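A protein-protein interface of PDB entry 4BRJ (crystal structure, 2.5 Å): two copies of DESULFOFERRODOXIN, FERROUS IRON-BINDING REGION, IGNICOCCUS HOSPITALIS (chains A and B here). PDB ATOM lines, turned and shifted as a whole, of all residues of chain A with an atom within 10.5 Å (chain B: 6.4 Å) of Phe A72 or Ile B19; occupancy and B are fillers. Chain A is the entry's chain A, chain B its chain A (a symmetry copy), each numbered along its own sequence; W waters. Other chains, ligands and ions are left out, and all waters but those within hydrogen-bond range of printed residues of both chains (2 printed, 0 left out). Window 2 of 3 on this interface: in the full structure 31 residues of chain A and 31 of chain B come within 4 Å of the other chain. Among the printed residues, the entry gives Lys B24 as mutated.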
ATOM      1  N   TYR A  64       5.325  39.433 -13.818  1.00  0.00           N
ATOM      2  CA  TYR A  64       5.864  38.388 -14.673  1.00  0.00           C
ATOM      3  C   TYR A  64       5.446  38.636 -16.126  1.00  0.00           C
ATOM      4  O   TYR A  64       4.600  39.494 -16.399  1.00  0.00           O
ATOM      5  CB  TYR A  64       5.317  37.026 -14.260  1.00  0.00           C
ATOM      6  CG  TYR A  64       5.808  36.432 -12.961  1.00  0.00           C
ATOM      7  CD1 TYR A  64       6.916  35.596 -12.940  1.00  0.00           C
ATOM      8  CD2 TYR A  64       5.127  36.657 -11.763  1.00  0.00           C
ATOM      9  CE1 TYR A  64       7.363  35.009 -11.764  1.00  0.00           C
ATOM     10  CE2 TYR A  64       5.564  36.083 -10.565  1.00  0.00           C
ATOM     11  CZ  TYR A  64       6.690  35.257 -10.570  1.00  0.00           C
ATOM     12  OH  TYR A  64       7.132  34.671  -9.390  1.00  0.00           O
ATOM     13  N   PHE A  65       6.024  37.858 -17.046  1.00  0.00           N
ATOM     14  CA  PHE A  65       5.769  38.015 -18.474  1.00  0.00           C
ATOM     15  C   PHE A  65       5.875  36.682 -19.212  1.00  0.00           C
ATOM     16  O   PHE A  65       6.874  35.952 -19.094  1.00  0.00           O
ATOM     17  CB  PHE A  65       6.734  39.036 -19.076  1.00  0.00           C
ATOM     18  CG  PHE A  65       6.524  39.305 -20.547  1.00  0.00           C
ATOM     19  CD1 PHE A  65       5.351  39.896 -21.006  1.00  0.00           C
ATOM     20  CD2 PHE A  65       7.530  39.006 -21.474  1.00  0.00           C
ATOM     21  CE1 PHE A  65       5.169  40.162 -22.371  1.00  0.00           C
ATOM     22  CE2 PHE A  65       7.363  39.269 -22.831  1.00  0.00           C
ATOM     23  CZ  PHE A  65       6.179  39.845 -23.284  1.00  0.00           C
ATOM     24  N   TYR A  66       4.819  36.357 -19.951  1.00  0.00           N
ATOM     25  CA  TYR A  66       4.835  35.221 -20.866  1.00  0.00           C
ATOM     26  C   TYR A  66       5.350  35.724 -22.219  1.00  0.00           C
ATOM     27  O   TYR A  66       4.703  36.532 -22.875  1.00  0.00           O
ATOM     28  CB  TYR A  66       3.427  34.621 -20.977  1.00  0.00           C
ATOM     29  CG  TYR A  66       3.325  33.409 -21.866  1.00  0.00           C
ATOM     30  CD1 TYR A  66       3.514  32.125 -21.358  1.00  0.00           C
ATOM     31  CD2 TYR A  66       3.022  33.538 -23.225  1.00  0.00           C
ATOM     32  CE1 TYR A  66       3.414  30.996 -22.198  1.00  0.00           C
ATOM     33  CE2 TYR A  66       2.915  32.422 -24.055  1.00  0.00           C
ATOM     34  CZ  TYR A  66       3.112  31.162 -23.536  1.00  0.00           C
ATOM     35  OH  TYR A  66       3.011  30.062 -24.365  1.00  0.00           O
ATOM     36  N   GLU A  67       6.539  35.296 -22.616  1.00  0.00           N
ATOM     37  CA  GLU A  67       7.093  35.741 -23.896  1.00  0.00           C
ATOM     38  C   GLU A  67       6.711  34.742 -24.983  1.00  0.00           C
ATOM     39  O   GLU A  67       7.114  33.581 -24.909  1.00  0.00           O
ATOM     40  CB  GLU A  67       8.612  35.864 -23.801  1.00  0.00           C
ATOM     41  CG  GLU A  67       9.277  36.588 -24.961  1.00  0.00           C
ATOM     42  CD  GLU A  67      10.682  37.057 -24.603  1.00  0.00           C
ATOM     43  OE1 GLU A  67      10.824  38.157 -24.012  1.00  0.00           O
ATOM     44  OE2 GLU A  67      11.644  36.312 -24.900  1.00  0.00           O
ATOM     45  N   GLU A  68       5.915  35.176 -25.964  1.00  0.00           N
ATOM     46  CA  GLU A  68       5.530  34.299 -27.083  1.00  0.00           C
ATOM     47  C   GLU A  68       6.773  33.783 -27.802  1.00  0.00           C
ATOM     48  O   GLU A  68       7.640  34.568 -28.197  1.00  0.00           O
ATOM     49  CB  GLU A  68       4.608  35.009 -28.093  1.00  0.00           C
ATOM     50  CG  GLU A  68       3.126  35.012 -27.738  1.00  0.00           C
ATOM     51  CD  GLU A  68       2.241  34.434 -28.852  1.00  0.00           C
ATOM     52  OE1 GLU A  68       2.516  34.670 -30.052  1.00  0.00           O
ATOM     53  OE2 GLU A  68       1.259  33.732 -28.525  1.00  0.00           O
ATOM     54  N   GLY A  69       6.869  32.465 -27.934  1.00  0.00           N
ATOM     55  CA  GLY A  69       7.959  31.850 -28.673  1.00  0.00           C
ATOM     56  C   GLY A  69       9.169  31.489 -27.822  1.00  0.00           C
ATOM     57  O   GLY A  69      10.031  30.717 -28.258  1.00  0.00           O
ATOM     58  N   ARG A  70       9.244  32.047 -26.616  1.00  0.00           N
ATOM     59  CA  ARG A  70      10.271  31.651 -25.663  1.00  0.00           C
ATOM     60  C   ARG A  70      10.046  30.181 -25.295  1.00  0.00           C
ATOM     61  O   ARG A  70       8.913  29.780 -25.034  1.00  0.00           O
ATOM     62  CB  ARG A  70      10.209  32.551 -24.414  1.00  0.00           C
ATOM     63  CG  ARG A  70      11.430  32.494 -23.495  1.00  0.00           C
ATOM     64  CD  ARG A  70      11.274  33.511 -22.393  1.00  0.00           C
ATOM     65  NE  ARG A  70      12.484  33.707 -21.603  1.00  0.00           N
ATOM     66  CZ  ARG A  70      12.812  32.999 -20.523  1.00  0.00           C
ATOM     67  NH1 ARG A  70      12.019  32.030 -20.082  1.00  0.00           N
ATOM     68  NH2 ARG A  70      13.934  33.278 -19.872  1.00  0.00           N
ATOM     69  N   PRO A  71      11.124  29.373 -25.280  1.00  0.00           N
ATOM     70  CA  PRO A  71      11.064  27.924 -25.014  1.00  0.00           C
ATOM     71  C   PRO A  71      10.376  27.581 -23.691  1.00  0.00           C
ATOM     72  O   PRO A  71       9.546  26.669 -23.628  1.00  0.00           O
ATOM     73  CB  PRO A  71      12.542  27.520 -24.934  1.00  0.00           C
ATOM     74  CG  PRO A  71      13.279  28.574 -25.633  1.00  0.00           C
ATOM     75  CD  PRO A  71      12.504  29.836 -25.501  1.00  0.00           C
ATOM     76  N   PHE A  72      10.755  28.305 -22.642  1.00  0.00           N
ATOM     77  CA  PHE A  72      10.148  28.172 -21.329  1.00  0.00           C
ATOM     78  C   PHE A  72       9.557  29.509 -20.921  1.00  0.00           C
ATOM     79  O   PHE A  72       9.906  30.541 -21.482  1.00  0.00           O
ATOM     80  CB  PHE A  72      11.168  27.676 -20.314  1.00  0.00           C
ATOM     81  CG  PHE A  72      11.687  26.291 -20.614  1.00  0.00           C
ATOM     82  CD1 PHE A  72      12.642  26.087 -21.614  1.00  0.00           C
ATOM     83  CD2 PHE A  72      11.222  25.193 -19.911  1.00  0.00           C
ATOM     84  CE1 PHE A  72      13.128  24.820 -21.892  1.00  0.00           C
ATOM     85  CE2 PHE A  72      11.702  23.916 -20.195  1.00  0.00           C
ATOM     86  CZ  PHE A  72      12.658  23.734 -21.188  1.00  0.00           C
ATOM     87  N   ASN A  73       8.622  29.479 -19.976  1.00  0.00           N
ATOM     88  CA  ASN A  73       7.929  30.682 -19.525  1.00  0.00           C
ATOM     89  C   ASN A  73       7.463  30.461 -18.086  1.00  0.00           C
ATOM     90  O   ASN A  73       7.409  29.308 -17.630  1.00  0.00           O
ATOM     91  CB  ASN A  73       6.739  30.983 -20.440  1.00  0.00           C
ATOM     92  CG  ASN A  73       7.054  32.039 -21.497  1.00  0.00           C
ATOM     93  OD1 ASN A  73       7.458  33.161 -21.172  1.00  0.00           O
ATOM     94  ND2 ASN A  73       6.852  31.687 -22.776  1.00  0.00           N
ATOM     95  N   PRO A  74       7.158  31.555 -17.354  1.00  0.00           N
ATOM     96  CA  PRO A  74       7.323  32.954 -17.756  1.00  0.00           C
ATOM     97  C   PRO A  74       8.674  33.519 -17.321  1.00  0.00           C
ATOM     98  O   PRO A  74       9.458  32.843 -16.656  1.00  0.00           O
ATOM     99  CB  PRO A  74       6.196  33.650 -16.996  1.00  0.00           C
ATOM    100  CG  PRO A  74       6.127  32.903 -15.721  1.00  0.00           C
ATOM    101  CD  PRO A  74       6.432  31.453 -16.077  1.00  0.00           C
ATOM    102  N   VAL A  75       8.942  34.751 -17.727  1.00  0.00           N
ATOM    103  CA  VAL A  75      10.074  35.498 -17.200  1.00  0.00           C
ATOM    104  C   VAL A  75       9.545  36.418 -16.114  1.00  0.00           C
ATOM    105  O   VAL A  75       8.609  37.179 -16.363  1.00  0.00           O
ATOM    106  CB  VAL A  75      10.704  36.415 -18.262  1.00  0.00           C
ATOM    107  CG1 VAL A  75      11.837  37.259 -17.648  1.00  0.00           C
ATOM    108  CG2 VAL A  75      11.222  35.616 -19.392  1.00  0.00           C
ATOM    109  N   MET A  76      10.131  36.359 -14.920  1.00  0.00           N
ATOM    110  CA  MET A  76       9.829  37.369 -13.905  1.00  0.00           C
ATOM    111  C   MET A  76      10.513  38.690 -14.237  1.00  0.00           C
ATOM    112  O   MET A  76      11.716  38.722 -14.425  1.00  0.00           O
ATOM    113  CB  MET A  76      10.264  36.923 -12.512  1.00  0.00           C
ATOM    114  CG  MET A  76       9.931  37.973 -11.468  1.00  0.00           C
ATOM    115  SD  MET A  76      10.598  37.609  -9.849  1.00  0.00           S
ATOM    116  CE  MET A  76       9.068  37.463  -8.926  1.00  0.00           C
ATOM    117  N   LYS A  99       9.717  40.930 -27.707  1.00  0.00           N
ATOM    118  CA  LYS A  99       8.694  40.075 -28.322  1.00  0.00           C
ATOM    119  C   LYS A  99       7.325  40.168 -27.629  1.00  0.00           C
ATOM    120  O   LYS A  99       7.237  40.504 -26.446  1.00  0.00           O
ATOM    121  CB  LYS A  99       9.179  38.621 -28.342  1.00  0.00           C
ATOM    122  CG  LYS A  99      10.186  38.335 -29.438  1.00  0.00           C
ATOM    123  CD  LYS A  99      10.889  37.003 -29.241  1.00  0.00           C
ATOM    124  CE  LYS A  99      11.812  36.711 -30.414  1.00  0.00           C
ATOM    125  NZ  LYS A  99      12.450  35.368 -30.313  1.00  0.00           N
ATOM    126  N   SER A 100       6.262  39.860 -28.368  1.00  0.00           N
ATOM    127  CA  SER A 100       4.898  39.927 -27.840  1.00  0.00           C
ATOM    128  C   SER A 100       4.600  38.894 -26.742  1.00  0.00           C
ATOM    129  O   SER A 100       5.220  37.828 -26.678  1.00  0.00           O
ATOM    130  CB  SER A 100       3.878  39.781 -28.965  1.00  0.00           C
ATOM    131  OG  SER A 100       3.938  40.876 -29.862  1.00  0.00           O
ATOM    132  N   TYR B   9       5.241  24.575 -13.693  1.00  0.00           N
ATOM    133  CA  TYR B   9       5.556  23.165 -13.829  1.00  0.00           C
ATOM    134  C   TYR B   9       5.263  22.404 -12.549  1.00  0.00           C
ATOM    135  O   TYR B   9       5.983  22.528 -11.570  1.00  0.00           O
ATOM    136  CB  TYR B   9       7.022  22.983 -14.253  1.00  0.00           C
ATOM    137  CG  TYR B   9       7.312  23.632 -15.585  1.00  0.00           C
ATOM    138  CD1 TYR B   9       7.143  22.930 -16.782  1.00  0.00           C
ATOM    139  CD2 TYR B   9       7.724  24.958 -15.653  1.00  0.00           C
ATOM    140  CE1 TYR B   9       7.388  23.537 -18.009  1.00  0.00           C
ATOM    141  CE2 TYR B   9       7.967  25.571 -16.864  1.00  0.00           C
ATOM    142  CZ  TYR B   9       7.799  24.861 -18.042  1.00  0.00           C
ATOM    143  OH  TYR B   9       8.047  25.488 -19.243  1.00  0.00           O
ATOM    144  N   GLU B  17       9.516  16.230 -19.159  1.00  0.00           N
ATOM    145  CA  GLU B  17      10.114  17.385 -19.826  1.00  0.00           C
ATOM    146  C   GLU B  17      11.515  17.047 -20.349  1.00  0.00           C
ATOM    147  O   GLU B  17      12.253  16.277 -19.729  1.00  0.00           O
ATOM    148  CB  GLU B  17      10.168  18.596 -18.881  1.00  0.00           C
ATOM    149  CG  GLU B  17       8.803  19.148 -18.465  1.00  0.00           C
ATOM    150  CD  GLU B  17       8.192  20.101 -19.490  1.00  0.00           C
ATOM    151  OE1 GLU B  17       8.963  20.743 -20.245  1.00  0.00           O
ATOM    152  OE2 GLU B  17       6.941  20.212 -19.535  1.00  0.00           O
ATOM    153  N   ALA B  18      11.864  17.626 -21.495  1.00  0.00           N
ATOM    154  CA  ALA B  18      13.160  17.397 -22.127  1.00  0.00           C
ATOM    155  C   ALA B  18      14.346  17.965 -21.329  1.00  0.00           C
ATOM    156  O   ALA B  18      15.471  17.485 -21.474  1.00  0.00           O
ATOM    157  CB  ALA B  18      13.154  17.955 -23.550  1.00  0.00           C
ATOM    158  N   ILE B  19      14.099  18.978 -20.495  1.00  0.00           N
ATOM    159  CA  ILE B  19      15.158  19.603 -19.689  1.00  0.00           C
ATOM    160  C   ILE B  19      15.425  18.848 -18.381  1.00  0.00           C
ATOM    161  O   ILE B  19      16.397  19.131 -17.682  1.00  0.00           O
ATOM    162  CB  ILE B  19      14.847  21.088 -19.351  1.00  0.00           C
ATOM    163  CG1 ILE B  19      16.138  21.872 -19.051  1.00  0.00           C
ATOM    164  CG2 ILE B  19      13.864  21.184 -18.178  1.00  0.00           C
ATOM    165  CD1 ILE B  19      17.083  22.055 -20.239  1.00  0.00           C
ATOM    166  N   SER B  20      14.559  17.893 -18.047  1.00  0.00           N
ATOM    167  CA  SER B  20      14.762  17.057 -16.860  1.00  0.00           C
ATOM    168  C   SER B  20      15.591  15.809 -17.205  1.00  0.00           C
ATOM    169  O   SER B  20      15.661  14.851 -16.428  1.00  0.00           O
ATOM    170  CB  SER B  20      13.427  16.679 -16.204  1.00  0.00           C
ATOM    171  OG  SER B  20      12.702  17.828 -15.792  1.00  0.00           O
ATOM    172  N   LYS B  21      16.205  15.834 -18.384  1.00  0.00           N
ATOM    173  CA  LYS B  21      17.232  14.868 -18.748  1.00  0.00           C
ATOM    174  C   LYS B  21      18.617  15.458 -18.470  1.00  0.00           C
ATOM    175  O   LYS B  21      19.625  14.760 -18.581  1.00  0.00           O
ATOM    176  CB  LYS B  21      17.142  14.494 -20.233  1.00  0.00           C
ATOM    177  CG  LYS B  21      15.883  13.761 -20.644  1.00  0.00           C
ATOM    178  CD  LYS B  21      15.897  13.488 -22.142  1.00  0.00           C
ATOM    179  CE  LYS B  21      14.587  12.881 -22.596  1.00  0.00           C
ATOM    180  NZ  LYS B  21      13.442  13.682 -22.078  1.00  0.00           N
ATOM    181  N   ALA B  22      18.661  16.743 -18.122  1.00  0.00           N
ATOM    182  CA  ALA B  22      19.928  17.449 -17.904  1.00  0.00           C
ATOM    183  C   ALA B  22      20.024  18.109 -16.520  1.00  0.00           C
ATOM    184  O   ALA B  22      21.124  18.306 -15.994  1.00  0.00           O
ATOM    185  CB  ALA B  22      20.157  18.487 -19.009  1.00  0.00           C
ATOM    186  N   GLU B  23      18.873  18.441 -15.938  1.00  0.00           N
ATOM    187  CA  GLU B  23      18.824  19.210 -14.694  1.00  0.00           C
ATOM    188  C   GLU B  23      17.435  19.198 -14.056  1.00  0.00           C
ATOM    189  O   GLU B  23      16.426  19.455 -14.717  1.00  0.00           O
ATOM    190  CB  GLU B  23      19.273  20.652 -14.951  1.00  0.00           C
ATOM    191  CG  GLU B  23      18.583  21.306 -16.142  1.00  0.00           C
ATOM    192  CD  GLU B  23      19.398  22.425 -16.762  1.00  0.00           C
ATOM    193  OE1 GLU B  23      20.345  22.127 -17.531  1.00  0.00           O
ATOM    194  OE2 GLU B  23      19.083  23.602 -16.487  1.00  0.00           O
ATOM    195  N   LYS B  24      17.391  18.891 -12.765  1.00  0.00           N
ATOM    196  CA  LYS B  24      16.132  18.877 -12.032  1.00  0.00           C
ATOM    197  C   LYS B  24      15.852  20.253 -11.428  1.00  0.00           C
ATOM    198  O   LYS B  24      16.711  20.846 -10.772  1.00  0.00           O
ATOM    199  CB  LYS B  24      16.151  17.800 -10.946  1.00  0.00           C
ATOM    200  CG  LYS B  24      16.713  16.480 -11.423  1.00  0.00           C
ATOM    201  CD  LYS B  24      16.025  16.010 -12.697  1.00  0.00           C
ATOM    202  CE  LYS B  24      16.901  15.021 -13.445  1.00  0.00           C
ATOM    203  NZ  LYS B  24      18.255  15.586 -13.710  1.00  0.00           N
ATOM    204  N   HIS B  25      14.653  20.768 -11.675  1.00  0.00           N
ATOM    205  CA  HIS B  25      14.276  22.079 -11.168  1.00  0.00           C
ATOM    206  C   HIS B  25      13.289  21.940 -10.021  1.00  0.00           C
ATOM    207  O   HIS B  25      13.098  22.870  -9.245  1.00  0.00           O
ATOM    208  CB  HIS B  25      13.634  22.930 -12.265  1.00  0.00           C
ATOM    209  CG  HIS B  25      14.577  23.365 -13.345  1.00  0.00           C
ATOM    210  ND1 HIS B  25      14.830  22.599 -14.464  1.00  0.00           N
ATOM    211  CD2 HIS B  25      15.296  24.503 -13.496  1.00  0.00           C
ATOM    212  CE1 HIS B  25      15.679  23.238 -15.249  1.00  0.00           C
ATOM    213  NE2 HIS B  25      15.977  24.396 -14.684  1.00  0.00           N
ATOM    214  N   HIS B  56      22.737  31.419 -15.782  1.00  0.00           N
ATOM    215  CA  HIS B  56      21.835  30.298 -15.549  1.00  0.00           C
ATOM    216  C   HIS B  56      21.921  29.755 -14.129  1.00  0.00           C
ATOM    217  O   HIS B  56      22.853  29.028 -13.793  1.00  0.00           O
ATOM    218  CB  HIS B  56      22.129  29.179 -16.555  1.00  0.00           C
ATOM    219  CG  HIS B  56      21.091  28.102 -16.587  1.00  0.00           C
ATOM    220  ND1 HIS B  56      21.170  27.022 -17.444  1.00  0.00           N
ATOM    221  CD2 HIS B  56      19.949  27.937 -15.880  1.00  0.00           C
ATOM    222  CE1 HIS B  56      20.127  26.234 -17.253  1.00  0.00           C
ATOM    223  NE2 HIS B  56      19.364  26.773 -16.322  1.00  0.00           N
ATOM    224  N   LEU B 111      16.043  30.799 -16.906  1.00  0.00           N
ATOM    225  CA  LEU B 111      15.760  30.283 -18.255  1.00  0.00           C
ATOM    226  C   LEU B 111      14.529  29.379 -18.275  1.00  0.00           C
ATOM    227  O   LEU B 111      13.776  29.345 -19.257  1.00  0.00           O
ATOM    228  CB  LEU B 111      16.948  29.503 -18.830  1.00  0.00           C
ATOM    229  CG  LEU B 111      18.283  30.220 -19.009  1.00  0.00           C
ATOM    230  CD1 LEU B 111      19.263  29.285 -19.697  1.00  0.00           C
ATOM    231  CD2 LEU B 111      18.111  31.509 -19.792  1.00  0.00           C
ATOM    232  N   HIS B 112      14.336  28.651 -17.181  1.00  0.00           N
ATOM    233  CA  HIS B 112      13.419  27.523 -17.184  1.00  0.00           C
ATOM    234  C   HIS B 112      12.120  27.712 -16.368  1.00  0.00           C
ATOM    235  O   HIS B 112      11.277  26.814 -16.299  1.00  0.00           O
ATOM    236  CB  HIS B 112      14.185  26.243 -16.834  1.00  0.00           C
ATOM    237  CG  HIS B 112      15.223  25.885 -17.854  1.00  0.00           C
ATOM    238  ND1 HIS B 112      16.457  25.367 -17.521  1.00  0.00           N
ATOM    239  CD2 HIS B 112      15.217  26.000 -19.205  1.00  0.00           C
ATOM    240  CE1 HIS B 112      17.160  25.169 -18.622  1.00  0.00           C
ATOM    241  NE2 HIS B 112      16.431  25.545 -19.657  1.00  0.00           N
ATOM    242  N   GLY B 113      11.947  28.898 -15.789  1.00  0.00           N
ATOM    243  CA  GLY B 113      10.684  29.275 -15.175  1.00  0.00           C
ATOM    244  C   GLY B 113      10.424  28.730 -13.783  1.00  0.00           C
ATOM    245  O   GLY B 113      11.361  28.530 -13.003  1.00  0.00           O
ATOM    246  N   TRP B 115       8.968  26.174 -10.864  1.00  0.00           N
ATOM    247  CA  TRP B 115       8.786  24.760 -10.539  1.00  0.00           C
ATOM    248  C   TRP B 115       8.290  24.541  -9.104  1.00  0.00           C
ATOM    249  O   TRP B 115       8.737  25.210  -8.158  1.00  0.00           O
ATOM    250  CB  TRP B 115      10.059  23.964 -10.849  1.00  0.00           C
ATOM    251  CG  TRP B 115      10.437  24.043 -12.315  1.00  0.00           C
ATOM    252  CD1 TRP B 115      10.837  25.160 -12.996  1.00  0.00           C
ATOM    253  CD2 TRP B 115      10.439  22.970 -13.276  1.00  0.00           C
ATOM    254  NE1 TRP B 115      11.086  24.852 -14.309  1.00  0.00           N
ATOM    255  CE2 TRP B 115      10.855  23.516 -14.508  1.00  0.00           C
ATOM    256  CE3 TRP B 115      10.148  21.607 -13.210  1.00  0.00           C
ATOM    257  CZ2 TRP B 115      10.980  22.744 -15.667  1.00  0.00           C
ATOM    258  CZ3 TRP B 115      10.270  20.843 -14.365  1.00  0.00           C
ATOM    259  CH2 TRP B 115      10.680  21.415 -15.574  1.00  0.00           C
HETATM  260  O   HOH W   1      13.919  29.555 -21.896  1.00  0.00           O
HETATM  261  O   HOH W   2      12.158  31.962 -17.026  1.00  0.00           O
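The backbone carbonyl oxygen of Leu B111 sits at hydrogen-bond distance from the guanidinium group of Arg A70 (3.3 Å).
The backbone carbonyl oxygen (O) of His B112 sits at hydrogen-bond distance from the indole nitrogen (NE1) of Trp B115.
The backbone carbonyl oxygen of Phe A72 lies within hydrogen-bond range of the guanidinium group of Arg A70, at 2.9 Å.
OE2 of Glu B23 lies close to ND1 of His B112 (3.3 Å).
OD1 of Asn A73 lies within hydrogen-bond range of N of Glu A67.
Among the printed residues, merely in contact across the chains: Phe A72 with Tyr B9 (3.3 Å), Phe A72 with Ile B19 (3.9 Å), Phe A72 with Leu B111 (3.3 Å), Phe A72 with His B112 (3.5 Å) and Asn A73 with Tyr B9 (3.9 Å).
Gly A69 touches none of the printed residues of chain B.
Printed residues of chain B within 4 Å of Arg A70: Leu B111 (3.3 Å).
Phe A72 touches just these residues of chain B: Tyr B9 (3.3 Å), Ile B19 (3.9 Å), Leu B111 (3.3 Å) and His B112 (3.5 Å).
Printed residues of chain B within 4 Å of Asn A73: Tyr B9.
No residue of chain A comes within 4 Å of Glu B17.
No residue of chain A comes within 4 Å of Ala B18.
Of the printed residues of chain A, Ile B19 touches Phe A72 (3.9 Å).
No residue of chain A comes within 4 Å of Ser B20.
Lys B21 touches none of the printed residues of chain A.
Of the printed residues of chain A, Leu B111 touches Arg A70 and Phe A72.
Of chain A, only Phe A72 (3.5 Å) comes within 4 Å of His B112.
The nearest residue of chain B that does not touch Phe A72 is Glu B17 (4.2 Å).
The nearest residue of chain A that does not touch Ile B19 is Pro A71 (8.5 Å).
The nearest printed residue of chain B that does not touch Asn A73 is Gly B113 (4.1 Å).
Of the 15 printed residues of chain A, 3 touch a printed residue of chain B.
Printed residues of chain A that touch a printed residue of chain B: Arg A70, Phe A72 and Asn A73.
Hydrophobic or aromatic side chains of chain A within 4 Å of the printed part of chain B: Phe A72.
Hydrophobic or aromatic side chains of chain B that line the printed part of chain A: Tyr B9, Ile B19 and His B112.
Among the printed residues, 6 pairs touch across the chains.
Among the printed residues, no Asp or Glu carboxylate lies within 4 Å of a Lys or Arg side-chain nitrogen of the other chain.
No position is printed for both chains.
Of the 6 pairs that touch across the chains among the printed residues, none has its exchanged pair printed and touching as well.
Water W1 lies within hydrogen-bond range of the backbone carbonyl oxygen of Leu B111 and the backbone NH of Phe A72.
Water W2 lies within hydrogen-bond range of the backbone carbonyl oxygen (O) of Pro A74, the guanidinium group (NH1) of Arg A70 and the backbone NH (N) of Gly B113.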
